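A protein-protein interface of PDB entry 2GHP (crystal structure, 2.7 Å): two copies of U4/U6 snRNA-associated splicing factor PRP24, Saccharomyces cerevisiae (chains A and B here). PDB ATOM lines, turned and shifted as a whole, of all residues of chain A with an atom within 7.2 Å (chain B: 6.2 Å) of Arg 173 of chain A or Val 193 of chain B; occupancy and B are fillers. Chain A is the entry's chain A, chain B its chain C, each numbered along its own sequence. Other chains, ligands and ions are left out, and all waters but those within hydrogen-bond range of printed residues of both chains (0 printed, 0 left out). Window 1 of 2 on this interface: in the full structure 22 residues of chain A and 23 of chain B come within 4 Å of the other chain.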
ATOM      1  N   GLU A 117      29.628  -2.075 -33.431  1.00  0.00           N
ATOM      2  CA  GLU A 117      29.394  -3.459 -32.979  1.00  0.00           C
ATOM      3  C   GLU A 117      28.940  -4.478 -34.044  1.00  0.00           C
ATOM      4  O   GLU A 117      28.179  -5.382 -33.738  1.00  0.00           O
ATOM      5  CB  GLU A 117      28.427  -3.445 -31.806  1.00  0.00           C
ATOM      6  CG  GLU A 117      29.100  -3.060 -30.533  1.00  0.00           C
ATOM      7  CD  GLU A 117      28.142  -2.606 -29.464  1.00  0.00           C
ATOM      8  OE1 GLU A 117      27.033  -2.153 -29.824  1.00  0.00           O
ATOM      9  OE2 GLU A 117      28.509  -2.688 -28.269  1.00  0.00           O
ATOM     10  N   LEU A 120      32.906  -9.551 -36.198  1.00  0.00           N
ATOM     11  CA  LEU A 120      33.255 -10.778 -35.534  1.00  0.00           C
ATOM     12  C   LEU A 120      34.560 -11.200 -36.108  1.00  0.00           C
ATOM     13  O   LEU A 120      34.896 -10.773 -37.194  1.00  0.00           O
ATOM     14  CB  LEU A 120      32.226 -11.866 -35.788  1.00  0.00           C
ATOM     15  CG  LEU A 120      31.707 -11.994 -37.209  1.00  0.00           C
ATOM     16  CD1 LEU A 120      31.412 -13.439 -37.608  1.00  0.00           C
ATOM     17  CD2 LEU A 120      30.457 -11.173 -37.304  1.00  0.00           C
ATOM     18  N   VAL A 166      29.567  -7.231 -40.710  1.00  0.00           N
ATOM     19  CA  VAL A 166      28.242  -7.512 -41.237  1.00  0.00           C
ATOM     20  C   VAL A 166      27.390  -6.223 -41.160  1.00  0.00           C
ATOM     21  O   VAL A 166      27.912  -5.143 -40.848  1.00  0.00           O
ATOM     22  CB  VAL A 166      27.619  -8.715 -40.533  1.00  0.00           C
ATOM     23  CG1 VAL A 166      28.364  -9.994 -40.895  1.00  0.00           C
ATOM     24  CG2 VAL A 166      27.654  -8.507 -39.034  1.00  0.00           C
ATOM     25  N   SER A 168      24.268  -5.557 -39.540  1.00  0.00           N
ATOM     26  CA  SER A 168      23.525  -5.189 -38.331  1.00  0.00           C
ATOM     27  C   SER A 168      24.069  -5.933 -37.157  1.00  0.00           C
ATOM     28  O   SER A 168      24.587  -7.049 -37.299  1.00  0.00           O
ATOM     29  CB  SER A 168      22.036  -5.487 -38.459  1.00  0.00           C
ATOM     30  OG  SER A 168      21.779  -6.881 -38.540  1.00  0.00           O
ATOM     31  N   LYS A 169      23.949  -5.294 -35.996  1.00  0.00           N
ATOM     32  CA  LYS A 169      24.287  -5.899 -34.702  1.00  0.00           C
ATOM     33  C   LYS A 169      23.683  -7.291 -34.517  1.00  0.00           C
ATOM     34  O   LYS A 169      24.393  -8.227 -34.153  1.00  0.00           O
ATOM     35  CB  LYS A 169      23.883  -4.966 -33.576  1.00  0.00           C
ATOM     36  CG  LYS A 169      24.651  -3.656 -33.611  1.00  0.00           C
ATOM     37  CD  LYS A 169      24.682  -2.948 -32.257  1.00  0.00           C
ATOM     38  CE  LYS A 169      23.918  -1.634 -32.306  1.00  0.00           C
ATOM     39  NZ  LYS A 169      24.250  -0.776 -31.121  1.00  0.00           N
ATOM     40  N   GLU A 170      22.391  -7.441 -34.810  1.00  0.00           N
ATOM     41  CA  GLU A 170      21.765  -8.753 -34.765  1.00  0.00           C
ATOM     42  C   GLU A 170      22.546  -9.751 -35.618  1.00  0.00           C
ATOM     43  O   GLU A 170      22.988 -10.794 -35.121  1.00  0.00           O
ATOM     44  CB  GLU A 170      20.314  -8.678 -35.215  1.00  0.00           C
ATOM     45  CG  GLU A 170      19.526  -9.965 -35.067  1.00  0.00           C
ATOM     46  CD  GLU A 170      19.910 -10.754 -33.817  1.00  0.00           C
ATOM     47  OE1 GLU A 170      19.917 -10.174 -32.703  1.00  0.00           O
ATOM     48  OE2 GLU A 170      20.216 -11.962 -33.949  1.00  0.00           O
ATOM     49  N   ASP A 171      22.739  -9.425 -36.892  1.00  0.00           N
ATOM     50  CA  ASP A 171      23.501 -10.298 -37.761  1.00  0.00           C
ATOM     51  C   ASP A 171      24.828 -10.780 -37.182  1.00  0.00           C
ATOM     52  O   ASP A 171      25.202 -11.915 -37.428  1.00  0.00           O
ATOM     53  CB  ASP A 171      23.720  -9.685 -39.140  1.00  0.00           C
ATOM     54  CG  ASP A 171      22.680 -10.131 -40.135  1.00  0.00           C
ATOM     55  OD1 ASP A 171      21.738 -10.841 -39.712  1.00  0.00           O
ATOM     56  OD2 ASP A 171      22.808  -9.797 -41.335  1.00  0.00           O
ATOM     57  N   ALA A 172      25.540  -9.943 -36.429  1.00  0.00           N
ATOM     58  CA  ALA A 172      26.803 -10.385 -35.828  1.00  0.00           C
ATOM     59  C   ALA A 172      26.554 -11.472 -34.760  1.00  0.00           C
ATOM     60  O   ALA A 172      27.166 -12.546 -34.786  1.00  0.00           O
ATOM     61  CB  ALA A 172      27.574  -9.212 -35.249  1.00  0.00           C
ATOM     62  N   ARG A 173      25.633 -11.202 -33.842  1.00  0.00           N
ATOM     63  CA  ARG A 173      25.286 -12.165 -32.818  1.00  0.00           C
ATOM     64  C   ARG A 173      24.744 -13.448 -33.465  1.00  0.00           C
ATOM     65  O   ARG A 173      25.165 -14.541 -33.120  1.00  0.00           O
ATOM     66  CB  ARG A 173      24.268 -11.567 -31.850  1.00  0.00           C
ATOM     67  CG  ARG A 173      24.721 -10.280 -31.197  1.00  0.00           C
ATOM     68  CD  ARG A 173      23.953  -9.927 -29.920  1.00  0.00           C
ATOM     69  NE  ARG A 173      24.159 -10.929 -28.865  1.00  0.00           N
ATOM     70  CZ  ARG A 173      23.895 -10.747 -27.566  1.00  0.00           C
ATOM     71  NH1 ARG A 173      23.444  -9.580 -27.119  1.00  0.00           N
ATOM     72  NH2 ARG A 173      24.090 -11.742 -26.705  1.00  0.00           N
ATOM     73  N   TYR A 174      23.822 -13.303 -34.418  1.00  0.00           N
ATOM     74  CA  TYR A 174      23.181 -14.437 -35.108  1.00  0.00           C
ATOM     75  C   TYR A 174      24.186 -15.329 -35.798  1.00  0.00           C
ATOM     76  O   TYR A 174      24.071 -16.552 -35.839  1.00  0.00           O
ATOM     77  CB  TYR A 174      22.255 -13.898 -36.177  1.00  0.00           C
ATOM     78  CG  TYR A 174      21.500 -14.967 -36.895  1.00  0.00           C
ATOM     79  CD1 TYR A 174      20.403 -15.593 -36.285  1.00  0.00           C
ATOM     80  CD2 TYR A 174      21.868 -15.370 -38.189  1.00  0.00           C
ATOM     81  CE1 TYR A 174      19.688 -16.595 -36.943  1.00  0.00           C
ATOM     82  CE2 TYR A 174      21.163 -16.379 -38.857  1.00  0.00           C
ATOM     83  CZ  TYR A 174      20.078 -16.988 -38.225  1.00  0.00           C
ATOM     84  OH  TYR A 174      19.357 -17.984 -38.855  1.00  0.00           O
ATOM     85  N   CYS A 175      25.169 -14.673 -36.363  1.00  0.00           N
ATOM     86  CA  CYS A 175      26.157 -15.294 -37.177  1.00  0.00           C
ATOM     87  C   CYS A 175      27.065 -16.167 -36.296  1.00  0.00           C
ATOM     88  O   CYS A 175      27.397 -17.327 -36.613  1.00  0.00           O
ATOM     89  CB  CYS A 175      26.913 -14.165 -37.838  1.00  0.00           C
ATOM     90  SG  CYS A 175      28.027 -14.697 -39.007  1.00  0.00           S
ATOM     91  N   VAL A 176      27.435 -15.613 -35.153  1.00  0.00           N
ATOM     92  CA  VAL A 176      28.202 -16.359 -34.169  1.00  0.00           C
ATOM     93  C   VAL A 176      27.376 -17.534 -33.644  1.00  0.00           C
ATOM     94  O   VAL A 176      27.865 -18.650 -33.527  1.00  0.00           O
ATOM     95  CB  VAL A 176      28.682 -15.440 -33.028  1.00  0.00           C
ATOM     96  CG1 VAL A 176      29.055 -16.243 -31.803  1.00  0.00           C
ATOM     97  CG2 VAL A 176      29.845 -14.641 -33.520  1.00  0.00           C
ATOM     98  N   GLU A 177      26.114 -17.303 -33.351  1.00  0.00           N
ATOM     99  CA  GLU A 177      25.304 -18.371 -32.796  1.00  0.00           C
ATOM    100  C   GLU A 177      25.099 -19.566 -33.739  1.00  0.00           C
ATOM    101  O   GLU A 177      25.092 -20.707 -33.294  1.00  0.00           O
ATOM    102  CB  GLU A 177      23.967 -17.842 -32.301  1.00  0.00           C
ATOM    103  CG  GLU A 177      23.487 -18.626 -31.111  1.00  0.00           C
ATOM    104  CD  GLU A 177      22.739 -17.765 -30.145  1.00  0.00           C
ATOM    105  OE1 GLU A 177      22.474 -16.573 -30.497  1.00  0.00           O
ATOM    106  OE2 GLU A 177      22.425 -18.291 -29.041  1.00  0.00           O
ATOM    107  N   LYS A 178      24.942 -19.301 -35.032  1.00  0.00           N
ATOM    108  CA  LYS A 178      24.796 -20.367 -36.006  1.00  0.00           C
ATOM    109  C   LYS A 178      26.115 -21.058 -36.320  1.00  0.00           C
ATOM    110  O   LYS A 178      26.122 -22.266 -36.591  1.00  0.00           O
ATOM    111  CB  LYS A 178      24.230 -19.817 -37.305  1.00  0.00           C
ATOM    112  CG  LYS A 178      22.745 -19.470 -37.276  1.00  0.00           C
ATOM    113  CD  LYS A 178      21.875 -20.710 -37.193  1.00  0.00           C
ATOM    114  CE  LYS A 178      20.796 -20.599 -38.194  1.00  0.00           C
ATOM    115  NZ  LYS A 178      19.681 -21.406 -37.719  1.00  0.00           N
ATOM    116  N   LEU A 179      27.220 -20.307 -36.327  1.00  0.00           N
ATOM    117  CA  LEU A 179      28.405 -20.849 -36.950  1.00  0.00           C
ATOM    118  C   LEU A 179      29.347 -21.468 -35.974  1.00  0.00           C
ATOM    119  O   LEU A 179      30.165 -22.316 -36.351  1.00  0.00           O
ATOM    120  CB  LEU A 179      29.124 -19.836 -37.823  1.00  0.00           C
ATOM    121  CG  LEU A 179      28.352 -19.371 -39.061  1.00  0.00           C
ATOM    122  CD1 LEU A 179      29.184 -18.308 -39.818  1.00  0.00           C
ATOM    123  CD2 LEU A 179      27.964 -20.513 -39.974  1.00  0.00           C
ATOM    124  N   VAL A 193      31.831 -12.510 -31.541  1.00  0.00           N
ATOM    125  CA  VAL A 193      31.724 -11.097 -31.804  1.00  0.00           C
ATOM    126  C   VAL A 193      33.007 -10.454 -31.269  1.00  0.00           C
ATOM    127  O   VAL A 193      33.551 -10.879 -30.271  1.00  0.00           O
ATOM    128  CB  VAL A 193      30.491 -10.502 -31.071  1.00  0.00           C
ATOM    129  CG1 VAL A 193      30.460  -9.029 -31.206  1.00  0.00           C
ATOM    130  CG2 VAL A 193      29.177 -11.097 -31.620  1.00  0.00           C
ATOM    131  N   GLU B 117      24.287  -1.495 -22.494  1.00  0.00           N
ATOM    132  CA  GLU B 117      24.931  -2.795 -22.737  1.00  0.00           C
ATOM    133  C   GLU B 117      25.558  -3.491 -21.532  1.00  0.00           C
ATOM    134  O   GLU B 117      26.509  -4.257 -21.681  1.00  0.00           O
ATOM    135  CB  GLU B 117      25.924  -2.714 -23.891  1.00  0.00           C
ATOM    136  CG  GLU B 117      25.259  -2.894 -25.228  1.00  0.00           C
ATOM    137  CD  GLU B 117      26.016  -2.247 -26.368  1.00  0.00           C
ATOM    138  OE1 GLU B 117      26.689  -1.209 -26.152  1.00  0.00           O
ATOM    139  OE2 GLU B 117      25.911  -2.769 -27.489  1.00  0.00           O
ATOM    140  N   THR B 119      23.582  -5.543 -19.325  1.00  0.00           N
ATOM    141  CA  THR B 119      22.511  -6.393 -18.793  1.00  0.00           C
ATOM    142  C   THR B 119      22.620  -7.846 -19.260  1.00  0.00           C
ATOM    143  O   THR B 119      22.659  -8.134 -20.454  1.00  0.00           O
ATOM    144  CB  THR B 119      21.111  -5.844 -19.176  1.00  0.00           C
ATOM    145  OG1 THR B 119      20.987  -4.476 -18.771  1.00  0.00           O
ATOM    146  CG2 THR B 119      19.988  -6.648 -18.545  1.00  0.00           C
ATOM    147  N   LEU B 120      22.671  -8.769 -18.320  1.00  0.00           N
ATOM    148  CA  LEU B 120      22.709 -10.175 -18.696  1.00  0.00           C
ATOM    149  C   LEU B 120      21.514 -10.890 -18.085  1.00  0.00           C
ATOM    150  O   LEU B 120      20.924 -10.384 -17.134  1.00  0.00           O
ATOM    151  CB  LEU B 120      24.023 -10.832 -18.261  1.00  0.00           C
ATOM    152  CG  LEU B 120      24.504 -10.534 -16.843  1.00  0.00           C
ATOM    153  CD1 LEU B 120      24.959 -11.789 -16.100  1.00  0.00           C
ATOM    154  CD2 LEU B 120      25.630  -9.515 -16.900  1.00  0.00           C
ATOM    155  N   TRP B 121      21.123 -12.032 -18.636  1.00  0.00           N
ATOM    156  CA  TRP B 121      20.164 -12.886 -17.937  1.00  0.00           C
ATOM    157  C   TRP B 121      20.868 -14.164 -17.534  1.00  0.00           C
ATOM    158  O   TRP B 121      21.854 -14.586 -18.154  1.00  0.00           O
ATOM    159  CB  TRP B 121      18.871 -13.151 -18.744  1.00  0.00           C
ATOM    160  CG  TRP B 121      19.147 -13.701 -20.108  1.00  0.00           C
ATOM    161  CD1 TRP B 121      19.288 -12.988 -21.249  1.00  0.00           C
ATOM    162  CD2 TRP B 121      19.370 -15.072 -20.459  1.00  0.00           C
ATOM    163  NE1 TRP B 121      19.581 -13.821 -22.298  1.00  0.00           N
ATOM    164  CE2 TRP B 121      19.641 -15.109 -21.840  1.00  0.00           C
ATOM    165  CE3 TRP B 121      19.378 -16.275 -19.739  1.00  0.00           C
ATOM    166  CZ2 TRP B 121      19.901 -16.311 -22.529  1.00  0.00           C
ATOM    167  CZ3 TRP B 121      19.649 -17.475 -20.429  1.00  0.00           C
ATOM    168  CH2 TRP B 121      19.903 -17.477 -21.802  1.00  0.00           C
ATOM    169  N   LYS B 169      30.380  -2.712 -19.726  1.00  0.00           N
ATOM    170  CA  LYS B 169      30.166  -3.639 -20.832  1.00  0.00           C
ATOM    171  C   LYS B 169      31.076  -4.874 -20.727  1.00  0.00           C
ATOM    172  O   LYS B 169      30.625  -6.011 -20.977  1.00  0.00           O
ATOM    173  CB  LYS B 169      30.305  -2.928 -22.185  1.00  0.00           C
ATOM    174  CG  LYS B 169      29.264  -1.835 -22.400  1.00  0.00           C
ATOM    175  CD  LYS B 169      29.284  -1.231 -23.805  1.00  0.00           C
ATOM    176  CE  LYS B 169      30.262  -0.053 -23.945  1.00  0.00           C
ATOM    177  NZ  LYS B 169      30.537   0.317 -25.382  1.00  0.00           N
ATOM    178  N   ALA B 172      29.838  -7.434 -18.099  1.00  0.00           N
ATOM    179  CA  ALA B 172      28.789  -8.290 -18.654  1.00  0.00           C
ATOM    180  C   ALA B 172      29.384  -9.491 -19.438  1.00  0.00           C
ATOM    181  O   ALA B 172      29.024 -10.643 -19.196  1.00  0.00           O
ATOM    182  CB  ALA B 172      27.847  -7.479 -19.518  1.00  0.00           C
ATOM    183  N   ARG B 173      30.315  -9.219 -20.346  1.00  0.00           N
ATOM    184  CA  ARG B 173      30.906 -10.281 -21.157  1.00  0.00           C
ATOM    185  C   ARG B 173      31.796 -11.248 -20.360  1.00  0.00           C
ATOM    186  O   ARG B 173      31.756 -12.464 -20.569  1.00  0.00           O
ATOM    187  CB  ARG B 173      31.650  -9.701 -22.360  1.00  0.00           C
ATOM    188  CG  ARG B 173      30.726  -8.913 -23.271  1.00  0.00           C
ATOM    189  CD  ARG B 173      31.470  -8.218 -24.380  1.00  0.00           C
ATOM    190  NE  ARG B 173      31.992  -9.204 -25.322  1.00  0.00           N
ATOM    191  CZ  ARG B 173      32.152  -8.996 -26.628  1.00  0.00           C
ATOM    192  NH1 ARG B 173      31.812  -7.836 -27.186  1.00  0.00           N
ATOM    193  NH2 ARG B 173      32.654  -9.960 -27.374  1.00  0.00           N
ATOM    194  N   VAL B 176      29.608 -13.508 -18.273  1.00  0.00           N
ATOM    195  CA  VAL B 176      29.059 -14.605 -19.065  1.00  0.00           C
ATOM    196  C   VAL B 176      30.139 -15.639 -19.412  1.00  0.00           C
ATOM    197  O   VAL B 176      29.918 -16.836 -19.290  1.00  0.00           O
ATOM    198  CB  VAL B 176      28.415 -14.052 -20.351  1.00  0.00           C
ATOM    199  CG1 VAL B 176      28.113 -15.164 -21.357  1.00  0.00           C
ATOM    200  CG2 VAL B 176      27.164 -13.263 -20.011  1.00  0.00           C
ATOM    201  N   THR B 191      24.007 -18.540 -18.784  1.00  0.00           N
ATOM    202  CA  THR B 191      24.005 -17.059 -18.869  1.00  0.00           C
ATOM    203  C   THR B 191      24.263 -16.571 -20.283  1.00  0.00           C
ATOM    204  O   THR B 191      24.957 -17.218 -21.065  1.00  0.00           O
ATOM    205  CB  THR B 191      25.118 -16.368 -18.045  1.00  0.00           C
ATOM    206  OG1 THR B 191      25.730 -17.269 -17.126  1.00  0.00           O
ATOM    207  CG2 THR B 191      24.566 -15.182 -17.310  1.00  0.00           C
ATOM    208  N   LYS B 192      23.742 -15.391 -20.593  1.00  0.00           N
ATOM    209  CA  LYS B 192      24.011 -14.705 -21.859  1.00  0.00           C
ATOM    210  C   LYS B 192      23.780 -13.225 -21.635  1.00  0.00           C
ATOM    211  O   LYS B 192      22.977 -12.822 -20.805  1.00  0.00           O
ATOM    212  CB  LYS B 192      23.101 -15.197 -23.006  1.00  0.00           C
ATOM    213  CG  LYS B 192      23.379 -16.633 -23.530  1.00  0.00           C
ATOM    214  CD  LYS B 192      24.339 -16.696 -24.717  1.00  0.00           C
ATOM    215  CE  LYS B 192      23.621 -16.472 -26.075  1.00  0.00           C
ATOM    216  NZ  LYS B 192      24.453 -16.932 -27.248  1.00  0.00           N
ATOM    217  N   VAL B 193      24.497 -12.411 -22.388  1.00  0.00           N
ATOM    218  CA  VAL B 193      24.258 -10.993 -22.380  1.00  0.00           C
ATOM    219  C   VAL B 193      22.895 -10.764 -23.023  1.00  0.00           C
ATOM    220  O   VAL B 193      22.513 -11.470 -23.961  1.00  0.00           O
ATOM    221  CB  VAL B 193      25.388 -10.266 -23.136  1.00  0.00           C
ATOM    222  CG1 VAL B 193      25.046  -8.788 -23.376  1.00  0.00           C
ATOM    223  CG2 VAL B 193      26.704 -10.446 -22.381  1.00  0.00           C
ATOM    224  N   SER B 194      22.156  -9.790 -22.505  1.00  0.00           N
ATOM    225  CA  SER B 194      20.883  -9.418 -23.088  1.00  0.00           C
ATOM    226  C   SER B 194      21.036  -8.907 -24.499  1.00  0.00           C
ATOM    227  O   SER B 194      22.004  -8.231 -24.822  1.00  0.00           O
ATOM    228  CB  SER B 194      20.214  -8.345 -22.273  1.00  0.00           C
ATOM    229  OG  SER B 194      18.865  -8.348 -22.643  1.00  0.00           O
ATOM    230  N   ASN B 195      20.065  -9.251 -25.336  1.00  0.00           N
ATOM    231  CA  ASN B 195      20.045  -8.848 -26.737  1.00  0.00           C
ATOM    232  C   ASN B 195      18.858  -7.898 -26.991  1.00  0.00           C
ATOM    233  O   ASN B 195      17.694  -8.321 -27.026  1.00  0.00           O
ATOM    234  CB  ASN B 195      20.004 -10.079 -27.637  1.00  0.00           C
ATOM    235  CG  ASN B 195      20.228  -9.748 -29.090  1.00  0.00           C
ATOM    236  OD1 ASN B 195      20.454  -8.585 -29.457  1.00  0.00           O
ATOM    237  ND2 ASN B 195      20.173 -10.766 -29.938  1.00  0.00           N
ATOM    238  N   PRO B 196      19.163  -6.598 -27.159  1.00  0.00           N
ATOM    239  CA  PRO B 196      18.149  -5.531 -27.147  1.00  0.00           C
ATOM    240  C   PRO B 196      17.309  -5.506 -28.414  1.00  0.00           C
ATOM    241  O   PRO B 196      17.777  -5.936 -29.467  1.00  0.00           O
ATOM    242  CB  PRO B 196      18.989  -4.256 -27.062  1.00  0.00           C
ATOM    243  CG  PRO B 196      20.298  -4.632 -27.736  1.00  0.00           C
ATOM    244  CD  PRO B 196      20.529  -6.079 -27.404  1.00  0.00           C
ATOM    245  N   ASP B 265      15.702 -12.409 -26.141  1.00  0.00           N
ATOM    246  CA  ASP B 265      16.193 -13.046 -24.946  1.00  0.00           C
ATOM    247  C   ASP B 265      15.413 -14.308 -24.697  1.00  0.00           C
ATOM    248  O   ASP B 265      15.983 -15.339 -24.338  1.00  0.00           O
ATOM    249  CB  ASP B 265      16.027 -12.121 -23.758  1.00  0.00           C
ATOM    250  CG  ASP B 265      17.180 -11.191 -23.583  1.00  0.00           C
ATOM    251  OD1 ASP B 265      18.048 -11.069 -24.474  1.00  0.00           O
ATOM    252  OD2 ASP B 265      17.213 -10.561 -22.529  1.00  0.00           O
ATOM    253  N   GLU B 268      16.463 -17.038 -26.895  1.00  0.00           N
ATOM    254  CA  GLU B 268      17.759 -17.569 -26.457  1.00  0.00           C
ATOM    255  C   GLU B 268      17.574 -18.496 -25.271  1.00  0.00           C
ATOM    256  O   GLU B 268      18.295 -19.469 -25.125  1.00  0.00           O
ATOM    257  CB  GLU B 268      18.706 -16.465 -26.010  1.00  0.00           C
ATOM    258  CG  GLU B 268      19.033 -15.448 -27.036  1.00  0.00           C
ATOM    259  CD  GLU B 268      19.979 -15.985 -28.064  1.00  0.00           C
ATOM    260  OE1 GLU B 268      20.602 -17.047 -27.785  1.00  0.00           O
ATOM    261  OE2 GLU B 268      20.089 -15.333 -29.137  1.00  0.00           O
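Printed residues of chain B within 4 Å of Arg 173 of chain A: Val 193, Ser 194 and Asn 195.
Printed residues of chain B within 4 Å of Glu 177 of chain A: Lys 192 and Glu 268.
Leu 120 of chain B touches none of the printed residues of chain A.
Lys 169 of chain B touches none of the printed residues of chain A.
Of the printed residues of chain A, Ser 194 of chain B touches Arg 173 (3.0 Å).
Of the printed residues of chain A, Glu 268 of chain B touches Glu 177.
The nearest printed residue of chain A that does not touch Lys 192 of chain B is Arg 173 of chain A (4.8 Å).
The side-chain amide nitrogen of Asn 195 of chain B lies within hydrogen-bond range of the side-chain carboxylate of Glu 170 of chain A (2.8 Å).
O of Val 193 of chain A lies within hydrogen-bond range of NH2 of Arg 173 of chain B.
The side-chain carboxylate (OE1) of Glu 117 of chain A lies close to the side-chain carboxylate (OE2) of Glu 117 of chain B (2.7 Å).
NH1 of Arg 173 of chain A is in hydrogen-bond range of O of Ser 194 of chain B, 3.0 Å away.
The backbone carbonyl oxygen (O) of Val 193 of chain B lies within hydrogen-bond range of the guanidinium group (NH2) of Arg 173 of chain A (3.2 Å).
The side-chain carboxylate (OE2) of Glu 177 of chain A is in salt-bridge range of the side-chain amino group (NZ) of Lys 192 of chain B (3.0 Å).
The side-chain carboxylate (OE1) of Glu 268 of chain B sits close to the side-chain carboxylate (OE2) of Glu 177 of chain A (2.5 Å).
Printed residues of chain A that touch a printed residue of chain B: Glu 117, Glu 170, Arg 173, Glu 177 and Val 193.
Along chain A the printed residues that touch a printed residue of chain B span positions 117 to 193.
Of the 16 printed residues of chain B, 7 touch a printed residue of chain A.
Among the printed residues, 8 pairs touch across the chains.
Among the printed residues, Asp or Glu carboxylates within 4 Å of a Lys or Arg side-chain nitrogen of the other chain: Glu 177 of chain A with Lys 192 of chain B.
N of Ser 194 of chain B is in hydrogen-bond range of O of Thr 119 of chain B (2.7 Å).
OG of Ser 194 of chain B lies within hydrogen-bond range of OD2 of Asp 265 of chain B (2.8 Å).
The backbone NH (N) of Asn 195 of chain B is in hydrogen-bond range of the side-chain carboxylate (OD1) of Asp 265 of chain B (2.8 Å).
The backbone carbonyl oxygen of Lys 192 of chain B lies within hydrogen-bond range of the backbone NH of Trp 121 of chain B (3.0 Å).
The side-chain amino group (NZ) of Lys 192 of chain B lies within salt-bridge range of the side-chain carboxylate (OE1) of Glu 268 of chain B, at 3.9 Å.
The side-chain amino group (NZ) of Lys 169 of chain A lies within salt-bridge range of the side-chain carboxylate (OE1) of Glu 117 of chain A.
Glu 117 of chain A touches its own counterpart, Glu 117 of chain B.
Arg 173 of chain A touches Val 193 of chain B, and with the chains exchanged Val 193 of chain A touches Arg 173 of chain B.
Among the printed residues, pairs that only touch across the chains: Arg 173 of chain A with Asn 195 of chain B.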
